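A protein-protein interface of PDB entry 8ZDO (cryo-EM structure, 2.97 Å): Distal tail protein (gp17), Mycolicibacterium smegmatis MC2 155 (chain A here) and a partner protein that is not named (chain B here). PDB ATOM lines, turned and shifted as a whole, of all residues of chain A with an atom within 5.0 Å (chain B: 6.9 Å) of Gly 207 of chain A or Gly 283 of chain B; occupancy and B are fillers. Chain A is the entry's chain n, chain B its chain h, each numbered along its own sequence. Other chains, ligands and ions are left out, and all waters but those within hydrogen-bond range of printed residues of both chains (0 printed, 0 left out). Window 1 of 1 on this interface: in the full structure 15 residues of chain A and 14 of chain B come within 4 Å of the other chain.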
ATOM      1  N   PHE A 192     -30.398 -18.854 -18.595  1.00  0.00           N
ATOM      2  CA  PHE A 192     -29.236 -19.165 -19.413  1.00  0.00           C
ATOM      3  C   PHE A 192     -29.541 -20.322 -20.351  1.00  0.00           C
ATOM      4  O   PHE A 192     -30.189 -21.299 -19.971  1.00  0.00           O
ATOM      5  CB  PHE A 192     -28.038 -19.520 -18.530  1.00  0.00           C
ATOM      6  CG  PHE A 192     -27.563 -18.396 -17.651  1.00  0.00           C
ATOM      7  CD1 PHE A 192     -28.143 -17.144 -17.714  1.00  0.00           C
ATOM      8  CD2 PHE A 192     -26.528 -18.599 -16.762  1.00  0.00           C
ATOM      9  CE1 PHE A 192     -27.707 -16.123 -16.904  1.00  0.00           C
ATOM     10  CE2 PHE A 192     -26.088 -17.579 -15.954  1.00  0.00           C
ATOM     11  CZ  PHE A 192     -26.678 -16.340 -16.028  1.00  0.00           C
ATOM     12  N   ASP A 205     -27.764 -16.203 -25.833  1.00  0.00           N
ATOM     13  CA  ASP A 205     -28.492 -16.273 -24.573  1.00  0.00           C
ATOM     14  C   ASP A 205     -27.676 -16.950 -23.476  1.00  0.00           C
ATOM     15  O   ASP A 205     -28.241 -17.537 -22.553  1.00  0.00           O
ATOM     16  CB  ASP A 205     -29.815 -17.011 -24.764  1.00  0.00           C
ATOM     17  CG  ASP A 205     -30.893 -16.136 -25.363  1.00  0.00           C
ATOM     18  OD1 ASP A 205     -30.772 -14.901 -25.282  1.00  0.00           O
ATOM     19  OD2 ASP A 205     -31.863 -16.688 -25.917  1.00  0.00           O
ATOM     20  N   LEU A 206     -26.346 -16.885 -23.569  1.00  0.00           N
ATOM     21  CA  LEU A 206     -25.507 -17.535 -22.567  1.00  0.00           C
ATOM     22  C   LEU A 206     -25.710 -16.919 -21.189  1.00  0.00           C
ATOM     23  O   LEU A 206     -25.755 -17.634 -20.183  1.00  0.00           O
ATOM     24  CB  LEU A 206     -24.037 -17.455 -22.977  1.00  0.00           C
ATOM     25  CG  LEU A 206     -23.517 -18.609 -23.834  1.00  0.00           C
ATOM     26  CD1 LEU A 206     -22.091 -18.349 -24.281  1.00  0.00           C
ATOM     27  CD2 LEU A 206     -23.612 -19.921 -23.083  1.00  0.00           C
ATOM     28  N   GLY A 207     -25.825 -15.598 -21.124  1.00  0.00           N
ATOM     29  CA  GLY A 207     -26.056 -14.923 -19.863  1.00  0.00           C
ATOM     30  C   GLY A 207     -27.385 -14.203 -19.837  1.00  0.00           C
ATOM     31  O   GLY A 207     -27.492 -13.095 -19.307  1.00  0.00           O
ATOM     32  N   ARG A 208     -28.407 -14.828 -20.410  1.00  0.00           N
ATOM     33  CA  ARG A 208     -29.719 -14.204 -20.495  1.00  0.00           C
ATOM     34  C   ARG A 208     -30.373 -14.140 -19.121  1.00  0.00           C
ATOM     35  O   ARG A 208     -30.390 -15.125 -18.380  1.00  0.00           O
ATOM     36  CB  ARG A 208     -30.602 -14.981 -21.469  1.00  0.00           C
ATOM     37  CG  ARG A 208     -32.069 -14.615 -21.417  1.00  0.00           C
ATOM     38  CD  ARG A 208     -32.846 -15.367 -22.477  1.00  0.00           C
ATOM     39  NE  ARG A 208     -34.056 -14.658 -22.872  1.00  0.00           N
ATOM     40  CZ  ARG A 208     -35.286 -15.092 -22.634  1.00  0.00           C
ATOM     41  NH1 ARG A 208     -35.507 -16.234 -22.006  1.00  0.00           N
ATOM     42  NH2 ARG A 208     -36.319 -14.358 -23.034  1.00  0.00           N
ATOM     43  N   THR A 209     -30.912 -12.976 -18.779  1.00  0.00           N
ATOM     44  CA  THR A 209     -31.691 -12.803 -17.563  1.00  0.00           C
ATOM     45  C   THR A 209     -33.029 -12.177 -17.917  1.00  0.00           C
ATOM     46  O   THR A 209     -33.094 -11.248 -18.726  1.00  0.00           O
ATOM     47  CB  THR A 209     -30.964 -11.930 -16.534  1.00  0.00           C
ATOM     48  OG1 THR A 209     -30.743 -10.625 -17.080  1.00  0.00           O
ATOM     49  CG2 THR A 209     -29.636 -12.550 -16.144  1.00  0.00           C
ATOM     50  N   PRO A 262     -27.122 -15.996 -11.327  1.00  0.00           N
ATOM     51  CA  PRO A 262     -27.433 -14.830 -10.493  1.00  0.00           C
ATOM     52  C   PRO A 262     -28.919 -14.553 -10.367  1.00  0.00           C
ATOM     53  O   PRO A 262     -29.648 -14.543 -11.363  1.00  0.00           O
ATOM     54  CB  PRO A 262     -26.723 -13.690 -11.225  1.00  0.00           C
ATOM     55  CG  PRO A 262     -26.773 -14.096 -12.651  1.00  0.00           C
ATOM     56  CD  PRO A 262     -26.718 -15.603 -12.688  1.00  0.00           C
ATOM     57  N   ARG B 169     -25.989  -3.356 -28.423  1.00  0.00           N
ATOM     58  CA  ARG B 169     -25.370  -4.375 -27.593  1.00  0.00           C
ATOM     59  C   ARG B 169     -24.717  -5.382 -28.532  1.00  0.00           C
ATOM     60  O   ARG B 169     -25.342  -5.818 -29.505  1.00  0.00           O
ATOM     61  CB  ARG B 169     -26.423  -5.045 -26.686  1.00  0.00           C
ATOM     62  CG  ARG B 169     -25.864  -6.020 -25.655  1.00  0.00           C
ATOM     63  CD  ARG B 169     -25.673  -7.438 -26.149  1.00  0.00           C
ATOM     64  NE  ARG B 169     -26.840  -8.128 -26.682  1.00  0.00           N
ATOM     65  CZ  ARG B 169     -27.736  -8.739 -25.923  1.00  0.00           C
ATOM     66  NH1 ARG B 169     -27.631  -8.754 -24.610  1.00  0.00           N
ATOM     67  NH2 ARG B 169     -28.739  -9.387 -26.494  1.00  0.00           N
ATOM     68  N   SER B 173     -21.763 -12.473 -25.715  1.00  0.00           N
ATOM     69  CA  SER B 173     -21.193 -12.040 -24.453  1.00  0.00           C
ATOM     70  C   SER B 173     -19.724 -12.432 -24.356  1.00  0.00           C
ATOM     71  O   SER B 173     -19.229 -13.281 -25.098  1.00  0.00           O
ATOM     72  CB  SER B 173     -21.972 -12.642 -23.286  1.00  0.00           C
ATOM     73  OG  SER B 173     -21.278 -12.466 -22.066  1.00  0.00           O
ATOM     74  N   CYS B 198     -19.535  -4.905 -18.940  1.00  0.00           N
ATOM     75  CA  CYS B 198     -20.137  -5.603 -17.803  1.00  0.00           C
ATOM     76  C   CYS B 198     -21.647  -5.388 -17.754  1.00  0.00           C
ATOM     77  O   CYS B 198     -22.234  -5.220 -16.684  1.00  0.00           O
ATOM     78  CB  CYS B 198     -19.483  -5.177 -16.488  1.00  0.00           C
ATOM     79  SG  CYS B 198     -17.822  -5.828 -16.237  1.00  0.00           S
ATOM     80  N   ALA B 199     -22.280  -5.394 -18.921  1.00  0.00           N
ATOM     81  CA  ALA B 199     -23.712  -5.179 -19.023  1.00  0.00           C
ATOM     82  C   ALA B 199     -24.466  -6.497 -18.905  1.00  0.00           C
ATOM     83  O   ALA B 199     -23.931  -7.576 -19.158  1.00  0.00           O
ATOM     84  CB  ALA B 199     -24.060  -4.497 -20.345  1.00  0.00           C
ATOM     85  N   ASP B 200     -25.729  -6.393 -18.510  1.00  0.00           N
ATOM     86  CA  ASP B 200     -26.606  -7.553 -18.454  1.00  0.00           C
ATOM     87  C   ASP B 200     -27.216  -7.777 -19.835  1.00  0.00           C
ATOM     88  O   ASP B 200     -26.838  -7.135 -20.819  1.00  0.00           O
ATOM     89  CB  ASP B 200     -27.663  -7.367 -17.372  1.00  0.00           C
ATOM     90  CG  ASP B 200     -28.462  -6.098 -17.553  1.00  0.00           C
ATOM     91  OD1 ASP B 200     -27.851  -5.039 -17.802  1.00  0.00           O
ATOM     92  OD2 ASP B 200     -29.706  -6.156 -17.446  1.00  0.00           O
ATOM     93  N   TYR B 201     -28.172  -8.703 -19.923  1.00  0.00           N
ATOM     94  CA  TYR B 201     -28.754  -9.048 -21.215  1.00  0.00           C
ATOM     95  C   TYR B 201     -29.463  -7.857 -21.847  1.00  0.00           C
ATOM     96  O   TYR B 201     -29.324  -7.611 -23.049  1.00  0.00           O
ATOM     97  CB  TYR B 201     -29.718 -10.219 -21.051  1.00  0.00           C
ATOM     98  CG  TYR B 201     -30.183 -10.812 -22.355  1.00  0.00           C
ATOM     99  CD1 TYR B 201     -29.348 -11.625 -23.102  1.00  0.00           C
ATOM    100  CD2 TYR B 201     -31.458 -10.564 -22.835  1.00  0.00           C
ATOM    101  CE1 TYR B 201     -29.766 -12.170 -24.291  1.00  0.00           C
ATOM    102  CE2 TYR B 201     -31.887 -11.104 -24.023  1.00  0.00           C
ATOM    103  CZ  TYR B 201     -31.037 -11.908 -24.747  1.00  0.00           C
ATOM    104  OH  TYR B 201     -31.462 -12.452 -25.936  1.00  0.00           O
ATOM    105  N   GLN B 202     -30.220  -7.105 -21.054  1.00  0.00           N
ATOM    106  CA  GLN B 202     -30.964  -5.953 -21.543  1.00  0.00           C
ATOM    107  C   GLN B 202     -30.225  -4.641 -21.325  1.00  0.00           C
ATOM    108  O   GLN B 202     -30.811  -3.574 -21.527  1.00  0.00           O
ATOM    109  CB  GLN B 202     -32.339  -5.892 -20.877  1.00  0.00           C
ATOM    110  CG  GLN B 202     -33.144  -7.172 -20.995  1.00  0.00           C
ATOM    111  CD  GLN B 202     -33.756  -7.344 -22.367  1.00  0.00           C
ATOM    112  OE1 GLN B 202     -33.990  -6.370 -23.081  1.00  0.00           O
ATOM    113  NE2 GLN B 202     -34.022  -8.586 -22.744  1.00  0.00           N
ATOM    114  N   HIS B 280     -21.369  -8.332 -11.214  1.00  0.00           N
ATOM    115  CA  HIS B 280     -20.360  -8.875 -12.110  1.00  0.00           C
ATOM    116  C   HIS B 280     -20.429 -10.393 -12.080  1.00  0.00           C
ATOM    117  O   HIS B 280     -20.848 -10.991 -11.086  1.00  0.00           O
ATOM    118  CB  HIS B 280     -18.950  -8.412 -11.730  1.00  0.00           C
ATOM    119  CG  HIS B 280     -18.769  -6.929 -11.778  1.00  0.00           C
ATOM    120  ND1 HIS B 280     -18.732  -6.221 -12.960  1.00  0.00           N
ATOM    121  CD2 HIS B 280     -18.619  -6.018 -10.789  1.00  0.00           C
ATOM    122  CE1 HIS B 280     -18.567  -4.937 -12.697  1.00  0.00           C
ATOM    123  NE2 HIS B 280     -18.495  -4.787 -11.387  1.00  0.00           N
ATOM    124  N   GLY B 281     -20.011 -11.010 -13.178  1.00  0.00           N
ATOM    125  CA  GLY B 281     -19.995 -12.456 -13.274  1.00  0.00           C
ATOM    126  C   GLY B 281     -20.801 -12.976 -14.444  1.00  0.00           C
ATOM    127  O   GLY B 281     -21.125 -12.218 -15.362  1.00  0.00           O
ATOM    128  N   GLU B 282     -21.129 -14.265 -14.423  1.00  0.00           N
ATOM    129  CA  GLU B 282     -21.938 -14.849 -15.484  1.00  0.00           C
ATOM    130  C   GLU B 282     -23.286 -14.148 -15.564  1.00  0.00           C
ATOM    131  O   GLU B 282     -23.946 -13.923 -14.546  1.00  0.00           O
ATOM    132  CB  GLU B 282     -22.129 -16.345 -15.244  1.00  0.00           C
ATOM    133  CG  GLU B 282     -20.855 -17.085 -14.880  1.00  0.00           C
ATOM    134  CD  GLU B 282     -20.701 -17.290 -13.383  1.00  0.00           C
ATOM    135  OE1 GLU B 282     -20.575 -16.285 -12.652  1.00  0.00           O
ATOM    136  OE2 GLU B 282     -20.702 -18.457 -12.940  1.00  0.00           O
ATOM    137  N   GLY B 283     -23.693 -13.800 -16.781  1.00  0.00           N
ATOM    138  CA  GLY B 283     -24.880 -13.010 -16.995  1.00  0.00           C
ATOM    139  C   GLY B 283     -24.654 -11.515 -16.990  1.00  0.00           C
ATOM    140  O   GLY B 283     -25.587 -10.764 -17.300  1.00  0.00           O
ATOM    141  N   PHE B 284     -23.452 -11.063 -16.652  1.00  0.00           N
ATOM    142  CA  PHE B 284     -23.096  -9.648 -16.605  1.00  0.00           C
ATOM    143  C   PHE B 284     -21.789  -9.414 -17.340  1.00  0.00           C
ATOM    144  O   PHE B 284     -20.874  -8.755 -16.844  1.00  0.00           O
ATOM    145  CB  PHE B 284     -22.998  -9.155 -15.167  1.00  0.00           C
ATOM    146  CG  PHE B 284     -24.222  -9.426 -14.354  1.00  0.00           C
ATOM    147  CD1 PHE B 284     -25.372  -8.684 -14.544  1.00  0.00           C
ATOM    148  CD2 PHE B 284     -24.224 -10.424 -13.401  1.00  0.00           C
ATOM    149  CE1 PHE B 284     -26.499  -8.935 -13.800  1.00  0.00           C
ATOM    150  CE2 PHE B 284     -25.348 -10.678 -12.656  1.00  0.00           C
ATOM    151  CZ  PHE B 284     -26.487  -9.933 -12.855  1.00  0.00           C
ATOM    152  N   ARG B 285     -21.684  -9.967 -18.545  1.00  0.00           N
ATOM    153  CA  ARG B 285     -20.476  -9.844 -19.346  1.00  0.00           C
ATOM    154  C   ARG B 285     -20.747  -9.295 -20.740  1.00  0.00           C
ATOM    155  O   ARG B 285     -19.844  -9.306 -21.581  1.00  0.00           O
ATOM    156  CB  ARG B 285     -19.765 -11.197 -19.445  1.00  0.00           C
ATOM    157  CG  ARG B 285     -19.141 -11.643 -18.144  1.00  0.00           C
ATOM    158  CD  ARG B 285     -18.918 -13.134 -18.120  1.00  0.00           C
ATOM    159  NE  ARG B 285     -18.221 -13.544 -16.908  1.00  0.00           N
ATOM    160  CZ  ARG B 285     -18.064 -14.802 -16.527  1.00  0.00           C
ATOM    161  NH1 ARG B 285     -18.548 -15.805 -17.239  1.00  0.00           N
ATOM    162  NH2 ARG B 285     -17.402 -15.062 -15.403  1.00  0.00           N
ATOM    163  N   TYR B 286     -21.957  -8.822 -21.008  1.00  0.00           N
ATOM    164  CA  TYR B 286     -22.248  -8.213 -22.294  1.00  0.00           C
ATOM    165  C   TYR B 286     -21.602  -6.834 -22.386  1.00  0.00           C
ATOM    166  O   TYR B 286     -21.220  -6.226 -21.384  1.00  0.00           O
ATOM    167  CB  TYR B 286     -23.757  -8.111 -22.505  1.00  0.00           C
ATOM    168  CG  TYR B 286     -24.428  -9.444 -22.732  1.00  0.00           C
ATOM    169  CD1 TYR B 286     -24.545  -9.970 -24.005  1.00  0.00           C
ATOM    170  CD2 TYR B 286     -24.939 -10.177 -21.672  1.00  0.00           C
ATOM    171  CE1 TYR B 286     -25.151 -11.186 -24.222  1.00  0.00           C
ATOM    172  CE2 TYR B 286     -25.547 -11.394 -21.878  1.00  0.00           C
ATOM    173  CZ  TYR B 286     -25.650 -11.894 -23.157  1.00  0.00           C
ATOM    174  OH  TYR B 286     -26.256 -13.107 -23.374  1.00  0.00           O
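The side-chain hydroxyl of Tyr 201 of chain B sits at hydrogen-bond distance from the side-chain carboxylate of Asp 205 of chain A (2.6 Å).
The backbone NH of Gly 207 of chain A is in hydrogen-bond range of the side-chain hydroxyl of Tyr 286 of chain B, 3.4 Å away.
The backbone carbonyl oxygen (O) of Tyr 286 of chain B lies within hydrogen-bond range of the backbone NH (N) of Cys 198 of chain B (3.2 Å).
The guanidinium group (NH1) of Arg 169 of chain B sits at hydrogen-bond distance from the backbone carbonyl oxygen (O) of Tyr 201 of chain B (2.6 Å).
N of Ala 199 of chain B sits at hydrogen-bond distance from O of Tyr 286 of chain B.
Among the printed residues, pairs that only touch across the chains: Phe 192 of chain A with Glu 282 of chain B, Phe 192 of chain A with Gly 283 of chain B, Leu 206 of chain A with Tyr 286 of chain B, Gly 207 of chain A with Gly 283 of chain B, Arg 208 of chain A with Tyr 201 of chain B, Thr 209 of chain A with Tyr 201 of chain B, Pro 262 of chain A with Glu 282 of chain B and Pro 262 of chain A with Phe 284 of chain B.
Printed residues of chain B within 4 Å of Phe 192 of chain A: Glu 282 (3.9 Å) and Gly 283 (3.9 Å).
Of chain B, only Gly 283 (3.5 Å) and Tyr 286 (3.4 Å) come within 4 Å of Gly 207 of chain A.
Printed residues of chain B within 4 Å of Pro 262 of chain A: Glu 282 (3.4 Å) and Phe 284 (3.6 Å).
Asp 200 of chain B touches none of the printed residues of chain A.
Of the printed residues of chain A, Glu 282 of chain B touches Phe 192 and Pro 262.
Of the printed residues of chain A, Gly 283 of chain B touches Phe 192 (3.9 Å) and Gly 207 (3.5 Å).
Printed residues of chain A within 4 Å of Phe 284 of chain B: Pro 262 (3.6 Å).
The nearest residue of chain B that does not touch Gly 207 of chain A is Tyr 201 of chain B (4.03 Å).
Hydrophobic or aromatic side chains of chain A within 4 Å of the printed part of chain B: Phe 192 and Pro 262.
Of the 14 printed residues of chain B, 5 touch a printed residue of chain A.
Hydrophobic or aromatic side chains of chain B within 4 Å of the printed part of chain A: Tyr 201, Phe 284 and Tyr 286.
Among the printed residues, no Asp or Glu carboxylate lies within 4 Å of a Lys or Arg side-chain nitrogen of the other chain.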
